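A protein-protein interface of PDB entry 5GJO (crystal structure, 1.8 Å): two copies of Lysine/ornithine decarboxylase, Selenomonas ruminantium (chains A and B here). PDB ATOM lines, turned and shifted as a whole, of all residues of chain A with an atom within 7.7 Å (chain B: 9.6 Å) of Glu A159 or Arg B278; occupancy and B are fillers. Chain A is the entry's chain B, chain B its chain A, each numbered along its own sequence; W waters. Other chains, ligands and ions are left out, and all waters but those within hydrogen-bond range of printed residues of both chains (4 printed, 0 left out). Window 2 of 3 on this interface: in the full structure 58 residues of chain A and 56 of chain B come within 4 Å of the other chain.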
ATOM      1  N   PHE A 116       4.949   0.493 -23.632  1.00  0.00           N
ATOM      2  CA  PHE A 116       4.982   1.931 -23.790  1.00  0.00           C
ATOM      3  C   PHE A 116       4.175   2.617 -22.695  1.00  0.00           C
ATOM      4  O   PHE A 116       3.352   2.008 -22.090  1.00  0.00           O
ATOM      5  CB  PHE A 116       4.524   2.350 -25.182  1.00  0.00           C
ATOM      6  CG  PHE A 116       3.042   2.243 -25.421  1.00  0.00           C
ATOM      7  CD1 PHE A 116       2.394   1.027 -25.343  1.00  0.00           C
ATOM      8  CD2 PHE A 116       2.312   3.352 -25.778  1.00  0.00           C
ATOM      9  CE1 PHE A 116       1.039   0.933 -25.575  1.00  0.00           C
ATOM     10  CE2 PHE A 116       0.968   3.260 -26.006  1.00  0.00           C
ATOM     11  CZ  PHE A 116       0.331   2.055 -25.905  1.00  0.00           C
ATOM     12  N   ASP A 117       4.486   3.875 -22.440  1.00  0.00           N
ATOM     13  CA  ASP A 117       3.754   4.651 -21.449  1.00  0.00           C
ATOM     14  C   ASP A 117       3.406   6.079 -21.877  1.00  0.00           C
ATOM     15  O   ASP A 117       2.962   6.860 -21.085  1.00  0.00           O
ATOM     16  CB  ASP A 117       4.464   4.605 -20.093  1.00  0.00           C
ATOM     17  CG  ASP A 117       5.844   5.239 -20.116  1.00  0.00           C
ATOM     18  OD1 ASP A 117       6.105   6.024 -21.022  1.00  0.00           O
ATOM     19  OD2 ASP A 117       6.634   4.933 -19.215  1.00  0.00           O
ATOM     20  N   ASP A 118       3.610   6.401 -23.144  1.00  0.00           N
ATOM     21  CA  ASP A 118       3.367   7.762 -23.602  1.00  0.00           C
ATOM     22  C   ASP A 118       2.870   7.808 -25.036  1.00  0.00           C
ATOM     23  O   ASP A 118       3.257   7.000 -25.832  1.00  0.00           O
ATOM     24  CB  ASP A 118       4.661   8.556 -23.500  1.00  0.00           C
ATOM     25  CG  ASP A 118       4.439  10.048 -23.560  1.00  0.00           C
ATOM     26  OD1 ASP A 118       4.189  10.617 -22.502  1.00  0.00           O
ATOM     27  OD2 ASP A 118       4.502  10.625 -24.644  1.00  0.00           O
ATOM     28  N   PRO A 119       2.052   8.784 -25.376  1.00  0.00           N
ATOM     29  CA  PRO A 119       1.638   8.822 -26.766  1.00  0.00           C
ATOM     30  C   PRO A 119       2.776   9.094 -27.763  1.00  0.00           C
ATOM     31  O   PRO A 119       2.684   8.682 -28.945  1.00  0.00           O
ATOM     32  CB  PRO A 119       0.662  10.010 -26.814  1.00  0.00           C
ATOM     33  CG  PRO A 119       0.887  10.768 -25.578  1.00  0.00           C
ATOM     34  CD  PRO A 119       1.361   9.791 -24.547  1.00  0.00           C
ATOM     35  N   SER A 120       3.867   9.733 -27.286  1.00  0.00           N
ATOM     36  CA  SER A 120       5.017  10.005 -28.186  1.00  0.00           C
ATOM     37  C   SER A 120       5.753   8.742 -28.568  1.00  0.00           C
ATOM     38  O   SER A 120       6.537   8.754 -29.468  1.00  0.00           O
ATOM     39  CB  SER A 120       5.935  11.047 -27.587  1.00  0.00           C
ATOM     40  OG  SER A 120       6.686  10.513 -26.494  1.00  0.00           O
ATOM     41  N   VAL A 136       0.507  -1.496 -22.629  1.00  0.00           N
ATOM     42  CA  VAL A 136       0.606  -0.147 -22.049  1.00  0.00           C
ATOM     43  C   VAL A 136       1.008  -0.315 -20.578  1.00  0.00           C
ATOM     44  O   VAL A 136       0.448  -1.111 -19.838  1.00  0.00           O
ATOM     45  CB  VAL A 136      -0.671   0.720 -22.179  1.00  0.00           C
ATOM     46  CG1 VAL A 136      -1.882   0.185 -21.410  1.00  0.00           C
ATOM     47  CG2 VAL A 136      -0.397   2.120 -21.715  1.00  0.00           C
ATOM     48  N   ARG A 137       2.024   0.398 -20.167  1.00  0.00           N
ATOM     49  CA  ARG A 137       2.492   0.366 -18.809  1.00  0.00           C
ATOM     50  C   ARG A 137       1.781   1.438 -17.987  1.00  0.00           C
ATOM     51  O   ARG A 137       1.843   2.609 -18.324  1.00  0.00           O
ATOM     52  CB  ARG A 137       4.015   0.604 -18.767  1.00  0.00           C
ATOM     53  CG  ARG A 137       4.585   0.528 -17.356  1.00  0.00           C
ATOM     54  CD  ARG A 137       6.082   0.614 -17.425  1.00  0.00           C
ATOM     55  NE  ARG A 137       6.732   0.673 -16.138  1.00  0.00           N
ATOM     56  CZ  ARG A 137       8.040   0.614 -15.953  1.00  0.00           C
ATOM     57  NH1 ARG A 137       8.841   0.214 -16.974  1.00  0.00           N
ATOM     58  NH2 ARG A 137       8.533   0.768 -14.724  1.00  0.00           N
ATOM     59  N   ILE A 138       1.138   1.046 -16.885  1.00  0.00           N
ATOM     60  CA  ILE A 138       0.471   1.970 -15.974  1.00  0.00           C
ATOM     61  C   ILE A 138       1.320   2.203 -14.737  1.00  0.00           C
ATOM     62  O   ILE A 138       2.063   1.329 -14.269  1.00  0.00           O
ATOM     63  CB  ILE A 138      -0.943   1.426 -15.480  1.00  0.00           C
ATOM     64  CG1 ILE A 138      -0.848   0.059 -14.880  1.00  0.00           C
ATOM     65  CG2 ILE A 138      -1.916   1.403 -16.651  1.00  0.00           C
ATOM     66  CD1 ILE A 138      -2.039  -0.400 -14.140  1.00  0.00           C
ATOM     67  N   THR A 151       7.559   6.989 -11.329  1.00  0.00           N
ATOM     68  CA  THR A 151       7.578   8.413 -11.621  1.00  0.00           C
ATOM     69  C   THR A 151       8.114   8.700 -13.025  1.00  0.00           C
ATOM     70  O   THR A 151       7.461   9.332 -13.833  1.00  0.00           O
ATOM     71  CB  THR A 151       8.432   9.151 -10.588  1.00  0.00           C
ATOM     72  OG1 THR A 151       7.857   8.966  -9.296  1.00  0.00           O
ATOM     73  CG2 THR A 151       8.498  10.643 -10.901  1.00  0.00           C
ATOM     74  N   LYS A 152       9.281   8.151 -13.311  1.00  0.00           N
ATOM     75  CA  LYS A 152       9.835   8.202 -14.671  1.00  0.00           C
ATOM     76  C   LYS A 152       9.094   7.382 -15.674  1.00  0.00           C
ATOM     77  O   LYS A 152       9.245   7.622 -16.880  1.00  0.00           O
ATOM     78  CB  LYS A 152      11.328   7.808 -14.668  1.00  0.00           C
ATOM     79  CG  LYS A 152      12.065   7.857 -16.022  1.00  0.00           C
ATOM     80  CD  LYS A 152      13.557   7.785 -15.791  1.00  0.00           C
ATOM     81  CE  LYS A 152      14.372   7.969 -17.055  1.00  0.00           C
ATOM     82  NZ  LYS A 152      14.287   6.875 -18.070  1.00  0.00           N
ATOM     83  N   PHE A 153       8.335   6.393 -15.212  1.00  0.00           N
ATOM     84  CA  PHE A 153       7.733   5.407 -16.054  1.00  0.00           C
ATOM     85  C   PHE A 153       6.255   5.238 -15.651  1.00  0.00           C
ATOM     86  O   PHE A 153       5.890   5.507 -14.524  1.00  0.00           O
ATOM     87  CB  PHE A 153       8.380   4.039 -15.837  1.00  0.00           C
ATOM     88  CG  PHE A 153       9.853   4.061 -15.897  1.00  0.00           C
ATOM     89  CD1 PHE A 153      10.494   4.111 -17.143  1.00  0.00           C
ATOM     90  CD2 PHE A 153      10.618   4.102 -14.779  1.00  0.00           C
ATOM     91  CE1 PHE A 153      11.864   4.175 -17.197  1.00  0.00           C
ATOM     92  CE2 PHE A 153      12.018   4.151 -14.858  1.00  0.00           C
ATOM     93  CZ  PHE A 153      12.627   4.158 -16.078  1.00  0.00           C
ATOM     94  N   GLY A 154       5.436   4.828 -16.604  1.00  0.00           N
ATOM     95  CA  GLY A 154       4.054   4.529 -16.304  1.00  0.00           C
ATOM     96  C   GLY A 154       3.086   5.622 -16.657  1.00  0.00           C
ATOM     97  O   GLY A 154       3.284   6.789 -16.277  1.00  0.00           O
ATOM     98  N   ALA A 155       2.022   5.282 -17.397  1.00  0.00           N
ATOM     99  CA  ALA A 155       1.004   6.273 -17.724  1.00  0.00           C
ATOM    100  C   ALA A 155      -0.040   6.348 -16.598  1.00  0.00           C
ATOM    101  O   ALA A 155      -0.301   5.318 -15.905  1.00  0.00           O
ATOM    102  CB  ALA A 155       0.302   5.932 -19.013  1.00  0.00           C
ATOM    103  N   PRO A 156      -0.656   7.484 -16.431  1.00  0.00           N
ATOM    104  CA  PRO A 156      -1.847   7.494 -15.526  1.00  0.00           C
ATOM    105  C   PRO A 156      -2.908   6.474 -15.948  1.00  0.00           C
ATOM    106  O   PRO A 156      -3.111   6.213 -17.141  1.00  0.00           O
ATOM    107  CB  PRO A 156      -2.394   8.916 -15.677  1.00  0.00           C
ATOM    108  CG  PRO A 156      -1.220   9.736 -16.192  1.00  0.00           C
ATOM    109  CD  PRO A 156      -0.420   8.806 -17.064  1.00  0.00           C
ATOM    110  N   VAL A 157      -3.501   5.781 -14.981  1.00  0.00           N
ATOM    111  CA  VAL A 157      -4.488   4.741 -15.302  1.00  0.00           C
ATOM    112  C   VAL A 157      -5.601   5.245 -16.186  1.00  0.00           C
ATOM    113  O   VAL A 157      -6.013   4.548 -17.089  1.00  0.00           O
ATOM    114  CB  VAL A 157      -5.078   4.054 -14.035  1.00  0.00           C
ATOM    115  CG1 VAL A 157      -4.010   3.298 -13.242  1.00  0.00           C
ATOM    116  CG2 VAL A 157      -5.706   5.055 -13.144  1.00  0.00           C
ATOM    117  N   GLU A 158      -6.029   6.502 -15.975  1.00  0.00           N
ATOM    118  CA  GLU A 158      -7.111   7.093 -16.756  1.00  0.00           C
ATOM    119  C   GLU A 158      -6.718   7.364 -18.222  1.00  0.00           C
ATOM    120  O   GLU A 158      -7.583   7.684 -19.061  1.00  0.00           O
ATOM    121  CB  GLU A 158      -7.695   8.355 -16.113  1.00  0.00           C
ATOM    122  CG  GLU A 158      -6.702   9.249 -15.391  1.00  0.00           C
ATOM    123  CD  GLU A 158      -6.349   8.692 -13.992  1.00  0.00           C
ATOM    124  OE1 GLU A 158      -5.196   8.339 -13.824  1.00  0.00           O
ATOM    125  OE2 GLU A 158      -7.231   8.532 -13.063  1.00  0.00           O
ATOM    126  N   GLU A 159      -5.445   7.191 -18.518  1.00  0.00           N
ATOM    127  CA  GLU A 159      -4.968   7.360 -19.862  1.00  0.00           C
ATOM    128  C   GLU A 159      -4.733   6.016 -20.560  1.00  0.00           C
ATOM    129  O   GLU A 159      -4.544   5.966 -21.747  1.00  0.00           O
ATOM    130  CB  GLU A 159      -3.698   8.211 -19.810  1.00  0.00           C
ATOM    131  CG  GLU A 159      -3.185   8.705 -21.136  1.00  0.00           C
ATOM    132  CD  GLU A 159      -1.989   9.630 -21.012  1.00  0.00           C
ATOM    133  OE1 GLU A 159      -1.829  10.261 -19.958  1.00  0.00           O
ATOM    134  OE2 GLU A 159      -1.250   9.738 -21.993  1.00  0.00           O
ATOM    135  N   ALA A 160      -4.762   4.923 -19.812  1.00  0.00           N
ATOM    136  CA  ALA A 160      -4.288   3.673 -20.371  1.00  0.00           C
ATOM    137  C   ALA A 160      -5.032   3.185 -21.614  1.00  0.00           C
ATOM    138  O   ALA A 160      -4.432   2.776 -22.657  1.00  0.00           O
ATOM    139  CB  ALA A 160      -4.350   2.599 -19.340  1.00  0.00           C
ATOM    140  N   LEU A 161      -6.351   3.114 -21.506  1.00  0.00           N
ATOM    141  CA  LEU A 161      -7.116   2.567 -22.596  1.00  0.00           C
ATOM    142  C   LEU A 161      -7.098   3.502 -23.791  1.00  0.00           C
ATOM    143  O   LEU A 161      -7.010   3.020 -24.938  1.00  0.00           O
ATOM    144  CB  LEU A 161      -8.542   2.204 -22.143  1.00  0.00           C
ATOM    145  CG  LEU A 161      -8.623   1.149 -21.063  1.00  0.00           C
ATOM    146  CD1 LEU A 161     -10.095   0.739 -20.858  1.00  0.00           C
ATOM    147  CD2 LEU A 161      -7.824  -0.080 -21.380  1.00  0.00           C
ATOM    148  N   ASP A 162      -7.104   4.787 -23.542  1.00  0.00           N
ATOM    149  CA  ASP A 162      -6.863   5.782 -24.647  1.00  0.00           C
ATOM    150  C   ASP A 162      -5.557   5.499 -25.389  1.00  0.00           C
ATOM    151  O   ASP A 162      -5.525   5.529 -26.646  1.00  0.00           O
ATOM    152  CB  ASP A 162      -6.895   7.201 -24.174  1.00  0.00           C
ATOM    153  CG  ASP A 162      -8.289   7.642 -23.678  1.00  0.00           C
ATOM    154  OD1 ASP A 162      -9.332   7.140 -24.217  1.00  0.00           O
ATOM    155  OD2 ASP A 162      -8.327   8.505 -22.754  1.00  0.00           O
ATOM    156  N   LEU A 163      -4.492   5.186 -24.637  1.00  0.00           N
ATOM    157  CA  LEU A 163      -3.231   4.879 -25.243  1.00  0.00           C
ATOM    158  C   LEU A 163      -3.275   3.607 -26.115  1.00  0.00           C
ATOM    159  O   LEU A 163      -2.717   3.589 -27.204  1.00  0.00           O
ATOM    160  CB  LEU A 163      -2.106   4.797 -24.186  1.00  0.00           C
ATOM    161  CG  LEU A 163      -1.638   6.113 -23.642  1.00  0.00           C
ATOM    162  CD1 LEU A 163      -0.845   5.911 -22.329  1.00  0.00           C
ATOM    163  CD2 LEU A 163      -0.756   6.796 -24.704  1.00  0.00           C
ATOM    164  N   LEU A 164      -3.946   2.561 -25.636  1.00  0.00           N
ATOM    165  CA  LEU A 164      -4.142   1.340 -26.416  1.00  0.00           C
ATOM    166  C   LEU A 164      -4.931   1.576 -27.708  1.00  0.00           C
ATOM    167  O   LEU A 164      -4.509   1.101 -28.774  1.00  0.00           O
ATOM    168  CB  LEU A 164      -4.781   0.300 -25.580  1.00  0.00           C
ATOM    169  CG  LEU A 164      -3.840  -0.277 -24.515  1.00  0.00           C
ATOM    170  CD1 LEU A 164      -4.568  -1.220 -23.587  1.00  0.00           C
ATOM    171  CD2 LEU A 164      -2.651  -1.002 -25.125  1.00  0.00           C
ATOM    172  N   LYS A 165      -5.915   2.456 -27.616  1.00  0.00           N
ATOM    173  CA  LYS A 165      -6.755   2.762 -28.776  1.00  0.00           C
ATOM    174  C   LYS A 165      -5.934   3.571 -29.792  1.00  0.00           C
ATOM    175  O   LYS A 165      -6.088   3.397 -31.000  1.00  0.00           O
ATOM    176  CB  LYS A 165      -8.014   3.524 -28.341  1.00  0.00           C
ATOM    177  CG  LYS A 165      -9.152   2.605 -27.871  1.00  0.00           C
ATOM    178  CD  LYS A 165      -9.964   3.064 -26.638  1.00  0.00           C
ATOM    179  CE  LYS A 165     -10.481   4.508 -26.653  1.00  0.00           C
ATOM    180  NZ  LYS A 165     -11.552   4.714 -27.667  1.00  0.00           N
ATOM    181  N   LEU A 201      -9.289  -2.275 -15.444  1.00  0.00           N
ATOM    182  CA  LEU A 201      -9.012  -1.827 -16.821  1.00  0.00           C
ATOM    183  C   LEU A 201      -9.344  -2.914 -17.859  1.00  0.00           C
ATOM    184  O   LEU A 201      -9.826  -2.595 -18.953  1.00  0.00           O
ATOM    185  CB  LEU A 201      -7.529  -1.356 -16.976  1.00  0.00           C
ATOM    186  CG  LEU A 201      -7.203  -0.096 -16.151  1.00  0.00           C
ATOM    187  CD1 LEU A 201      -5.712   0.228 -16.173  1.00  0.00           C
ATOM    188  CD2 LEU A 201      -7.903   1.147 -16.635  1.00  0.00           C
ATOM    189  N   THR B 275       9.260  12.373 -25.268  1.00  0.00           N
ATOM    190  CA  THR B 275       8.688  13.428 -24.474  1.00  0.00           C
ATOM    191  C   THR B 275       7.558  12.874 -23.600  1.00  0.00           C
ATOM    192  O   THR B 275       6.991  11.782 -23.869  1.00  0.00           O
ATOM    193  CB  THR B 275       8.083  14.527 -25.315  1.00  0.00           C
ATOM    194  OG1 THR B 275       7.015  13.993 -26.132  1.00  0.00           O
ATOM    195  CG2 THR B 275       9.153  15.134 -26.268  1.00  0.00           C
ATOM    196  N   LYS B 276       7.258  13.599 -22.534  1.00  0.00           N
ATOM    197  CA  LYS B 276       6.069  13.382 -21.732  1.00  0.00           C
ATOM    198  C   LYS B 276       5.471  14.758 -21.490  1.00  0.00           C
ATOM    199  O   LYS B 276       5.962  15.492 -20.679  1.00  0.00           O
ATOM    200  CB  LYS B 276       6.438  12.690 -20.429  1.00  0.00           C
ATOM    201  CG  LYS B 276       7.159  11.378 -20.640  1.00  0.00           C
ATOM    202  CD  LYS B 276       7.716  10.805 -19.367  1.00  0.00           C
ATOM    203  CE  LYS B 276       8.464   9.510 -19.617  1.00  0.00           C
ATOM    204  NZ  LYS B 276       7.854   8.580 -20.604  1.00  0.00           N
ATOM    205  N   THR B 277       4.420  15.093 -22.219  1.00  0.00           N
ATOM    206  CA  THR B 277       3.822  16.422 -22.119  1.00  0.00           C
ATOM    207  C   THR B 277       2.649  16.530 -21.152  1.00  0.00           C
ATOM    208  O   THR B 277       2.122  17.628 -20.926  1.00  0.00           O
ATOM    209  CB  THR B 277       3.353  16.920 -23.493  1.00  0.00           C
ATOM    210  OG1 THR B 277       2.400  15.985 -24.023  1.00  0.00           O
ATOM    211  CG2 THR B 277       4.530  17.055 -24.460  1.00  0.00           C
ATOM    212  N   ARG B 278       2.220  15.418 -20.558  1.00  0.00           N
ATOM    213  CA  ARG B 278       1.037  15.458 -19.728  1.00  0.00           C
ATOM    214  C   ARG B 278       1.308  16.315 -18.492  1.00  0.00           C
ATOM    215  O   ARG B 278       2.430  16.386 -17.984  1.00  0.00           O
ATOM    216  CB  ARG B 278       0.664  14.011 -19.299  1.00  0.00           C
ATOM    217  CG  ARG B 278       1.609  13.343 -18.275  1.00  0.00           C
ATOM    218  CD  ARG B 278       0.956  12.027 -17.828  1.00  0.00           C
ATOM    219  NE  ARG B 278       0.747  11.130 -18.946  1.00  0.00           N
ATOM    220  CZ  ARG B 278       1.652  10.253 -19.391  1.00  0.00           C
ATOM    221  NH1 ARG B 278       1.390   9.438 -20.416  1.00  0.00           N
ATOM    222  NH2 ARG B 278       2.858  10.211 -18.850  1.00  0.00           N
ATOM    223  N   GLY B 279       0.295  16.951 -17.937  1.00  0.00           N
ATOM    224  CA  GLY B 279       0.642  17.784 -16.765  1.00  0.00           C
ATOM    225  C   GLY B 279       1.604  18.992 -16.925  1.00  0.00           C
ATOM    226  O   GLY B 279       1.903  19.454 -18.045  1.00  0.00           O
ATOM    227  N   GLU B 280       2.054  19.540 -15.799  1.00  0.00           N
ATOM    228  CA  GLU B 280       2.583  20.921 -15.846  1.00  0.00           C
ATOM    229  C   GLU B 280       4.064  21.013 -16.193  1.00  0.00           C
ATOM    230  O   GLU B 280       4.484  21.960 -16.827  1.00  0.00           O
ATOM    231  CB  GLU B 280       2.299  21.692 -14.557  1.00  0.00           C
ATOM    232  CG  GLU B 280       2.254  23.207 -14.752  1.00  0.00           C
ATOM    233  CD  GLU B 280       1.607  23.906 -13.563  1.00  0.00           C
ATOM    234  OE1 GLU B 280       0.519  24.520 -13.751  1.00  0.00           O
ATOM    235  OE2 GLU B 280       2.171  23.810 -12.437  1.00  0.00           O
ATOM    236  N   GLN B 281       4.835  20.036 -15.758  1.00  0.00           N
ATOM    237  CA  GLN B 281       6.255  20.007 -16.080  1.00  0.00           C
ATOM    238  C   GLN B 281       6.542  18.958 -17.193  1.00  0.00           C
ATOM    239  O   GLN B 281       6.473  17.796 -16.952  1.00  0.00           O
ATOM    240  CB  GLN B 281       7.021  19.790 -14.789  1.00  0.00           C
ATOM    241  CG  GLN B 281       8.485  19.563 -14.998  1.00  0.00           C
ATOM    242  CD  GLN B 281       9.396  20.056 -13.939  1.00  0.00           C
ATOM    243  OE1 GLN B 281      10.560  19.787 -13.996  1.00  0.00           O
ATOM    244  NE2 GLN B 281       8.890  20.852 -12.996  1.00  0.00           N
ATOM    245  N   PRO B 282       6.895  19.382 -18.410  1.00  0.00           N
ATOM    246  CA  PRO B 282       7.222  18.371 -19.380  1.00  0.00           C
ATOM    247  C   PRO B 282       8.473  17.596 -19.006  1.00  0.00           C
ATOM    248  O   PRO B 282       9.399  18.167 -18.362  1.00  0.00           O
ATOM    249  CB  PRO B 282       7.509  19.150 -20.644  1.00  0.00           C
ATOM    250  CG  PRO B 282       7.491  20.554 -20.322  1.00  0.00           C
ATOM    251  CD  PRO B 282       7.111  20.728 -18.896  1.00  0.00           C
ATOM    252  N   TRP B 283       8.559  16.359 -19.480  1.00  0.00           N
ATOM    253  CA  TRP B 283       9.789  15.550 -19.382  1.00  0.00           C
ATOM    254  C   TRP B 283      10.332  15.307 -20.758  1.00  0.00           C
ATOM    255  O   TRP B 283       9.597  15.062 -21.738  1.00  0.00           O
ATOM    256  CB  TRP B 283       9.585  14.211 -18.766  1.00  0.00           C
ATOM    257  CG  TRP B 283       9.339  14.175 -17.298  1.00  0.00           C
ATOM    258  CD1 TRP B 283       8.425  14.917 -16.588  1.00  0.00           C
ATOM    259  CD2 TRP B 283       9.974  13.314 -16.330  1.00  0.00           C
ATOM    260  NE1 TRP B 283       8.516  14.615 -15.236  1.00  0.00           N
ATOM    261  CE2 TRP B 283       9.399  13.587 -15.072  1.00  0.00           C
ATOM    262  CE3 TRP B 283      10.969  12.348 -16.402  1.00  0.00           C
ATOM    263  CZ2 TRP B 283       9.850  12.969 -13.898  1.00  0.00           C
ATOM    264  CZ3 TRP B 283      11.415  11.762 -15.247  1.00  0.00           C
ATOM    265  CH2 TRP B 283      10.826  12.035 -14.008  1.00  0.00           C
ATOM    266  N   TYR B 284      11.641  15.299 -20.837  1.00  0.00           N
ATOM    267  CA  TYR B 284      12.339  14.877 -22.003  1.00  0.00           C
ATOM    268  C   TYR B 284      13.295  13.753 -21.632  1.00  0.00           C
ATOM    269  O   TYR B 284      14.084  13.899 -20.690  1.00  0.00           O
ATOM    270  CB  TYR B 284      13.175  16.024 -22.531  1.00  0.00           C
ATOM    271  CG  TYR B 284      12.291  17.211 -22.807  1.00  0.00           C
ATOM    272  CD1 TYR B 284      11.375  17.129 -23.840  1.00  0.00           C
ATOM    273  CD2 TYR B 284      12.352  18.361 -22.050  1.00  0.00           C
ATOM    274  CE1 TYR B 284      10.508  18.162 -24.096  1.00  0.00           C
ATOM    275  CE2 TYR B 284      11.528  19.473 -22.350  1.00  0.00           C
ATOM    276  CZ  TYR B 284      10.592  19.321 -23.355  1.00  0.00           C
ATOM    277  OH  TYR B 284       9.776  20.326 -23.749  1.00  0.00           O
ATOM    278  N   LYS B 315       9.760  26.763 -20.076  1.00  0.00           N
ATOM    279  CA  LYS B 315       9.138  26.457 -18.812  1.00  0.00           C
ATOM    280  C   LYS B 315       9.916  25.371 -18.044  1.00  0.00           C
ATOM    281  O   LYS B 315      10.693  24.595 -18.694  1.00  0.00           O
ATOM    282  CB  LYS B 315       7.716  25.988 -19.084  1.00  0.00           C
ATOM    283  CG  LYS B 315       7.570  24.739 -19.859  1.00  0.00           C
ATOM    284  CD  LYS B 315       6.115  24.246 -19.907  1.00  0.00           C
ATOM    285  CE  LYS B 315       5.295  25.143 -20.791  1.00  0.00           C
ATOM    286  NZ  LYS B 315       3.925  24.542 -20.856  1.00  0.00           N
ATOM    287  N   PRO B 316       9.664  25.262 -16.738  1.00  0.00           N
ATOM    288  CA  PRO B 316      10.415  24.271 -15.993  1.00  0.00           C
ATOM    289  C   PRO B 316      10.147  22.902 -16.489  1.00  0.00           C
ATOM    290  O   PRO B 316       8.941  22.491 -16.669  1.00  0.00           O
ATOM    291  CB  PRO B 316       9.936  24.473 -14.502  1.00  0.00           C
ATOM    292  CG  PRO B 316       9.574  25.923 -14.489  1.00  0.00           C
ATOM    293  CD  PRO B 316       8.905  26.157 -15.811  1.00  0.00           C
HETATM  294  O   HOH W   1       4.489  13.283 -24.779  1.00  0.00           O
HETATM  295  O   HOH W   2       9.068   6.335 -19.405  1.00  0.00           O
HETATM  296  O   HOH W   3       4.961   8.736 -20.175  1.00  0.00           O
HETATM  297  O   HOH W   4       2.614  12.632 -21.802  1.00  0.00           O
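Water W4 lies within hydrogen-bond range of the side-chain carboxylate of Asp A118 (2.7 Å), the backbone NH of Arg B278 (3.1 Å) and the backbone NH of Thr B277 (3.1 Å).
Water W1 lies within hydrogen-bond range of the side-chain carboxylate (OD2) of Asp A118, the side-chain hydroxyl (OG1) of Thr B275 and the backbone NH (N) of Thr B277.
Water W2 lies within hydrogen-bond range of the side-chain carboxylate of Asp A117 (2.8 Å), the side-chain amino group of Lys B276 (2.8 Å) and the backbone carbonyl oxygen of Lys A152 (2.8 Å).
Water W3 lies within hydrogen-bond range of O of Asp A117 (2.9 Å), NH2 of Arg B278 (2.9 Å), NZ of Lys B276 (2.9 Å) and OD1 of Asp A118 (3.1 Å).
The side-chain hydroxyl (OG) of Ser A120 lies within hydrogen-bond range of the backbone carbonyl oxygen (O) of Thr B275, 2.9 Å away.
The side-chain carboxylate (OD1) of Asp A117 is in salt-bridge range of the side-chain amino group (NZ) of Lys B276.
NH1 of Arg B278 sits at hydrogen-bond distance from O of Asp A117 (3.1 Å).
The guanidinium group of Arg B278 is in salt-bridge range of the side-chain carboxylate of Asp A118 (3.7 Å).
The side-chain carboxylate (OE1) of Glu A159 is in salt-bridge range of the guanidinium group (NE) of Arg B278.
The side-chain carboxylate of Asp A118 lies close to the backbone carbonyl oxygen of Thr B275.
No position is printed for both chains.
Among the printed residues, merely in contact across the chains: Asp A118 with Lys B276 (3.4 Å), Lys A152 with Lys B276 (3.4 Å), Lys A152 with Trp B283 (3.9 Å), Ala A155 with Arg B278 (3.9 Å) and Pro A156 with Arg B278 (3.2 Å).
Of the 12 printed residues of chain B, 4 touch a printed residue of chain A.
Hydrophobic or aromatic side chains of chain B within 4 Å of the printed part of chain A: Trp B283.
Hydrophobic or aromatic side chains of chain A within 4 Å of the printed part of chain B: Ala A155 and Pro A156.
Among the printed residues, 11 pairs touch across the chains.
Among the printed residues, Asp or Glu carboxylates within 4 Å of a Lys or Arg side-chain nitrogen of the other chain: Asp A117 with Lys B276, Asp A118 with Arg B278 and Glu A159 with Arg B278.
Glu A159 touches just one residue of chain B: Arg B278 (2.9 Å).
Arg B278 touches five residues of chain A.
Pro A156 touches one residue of chain B.
No residue of chain B comes within 4 Å of Ala A160.
No residue of chain B comes within 4 Å of Asp A162.
No residue of chain A comes within 4 Å of Gly B279.
Printed residues of chain B within 4 Å of Ala A155: Arg B278.
Of the printed residues of chain A, Trp B283 touches Lys A152.
Gly A154 touches none of the printed residues of chain B.
The nearest printed residue of chain A that does not touch Lys B276 is Ser A120 (5.1 Å).
The backbone NH of Lys B276 sits at hydrogen-bond distance from the backbone carbonyl oxygen of Trp B283 (2.9 Å).
OD2 of Asp A117 lies within hydrogen-bond range of N of Gly A154 (2.9 Å).
The backbone NH (N) of Ser A120 lies within hydrogen-bond range of the side-chain carboxylate (OD2) of Asp A118 (2.9 Å).
The backbone NH (N) of Ala A155 lies within hydrogen-bond range of the backbone carbonyl oxygen (O) of Arg A137 (2.8 Å).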
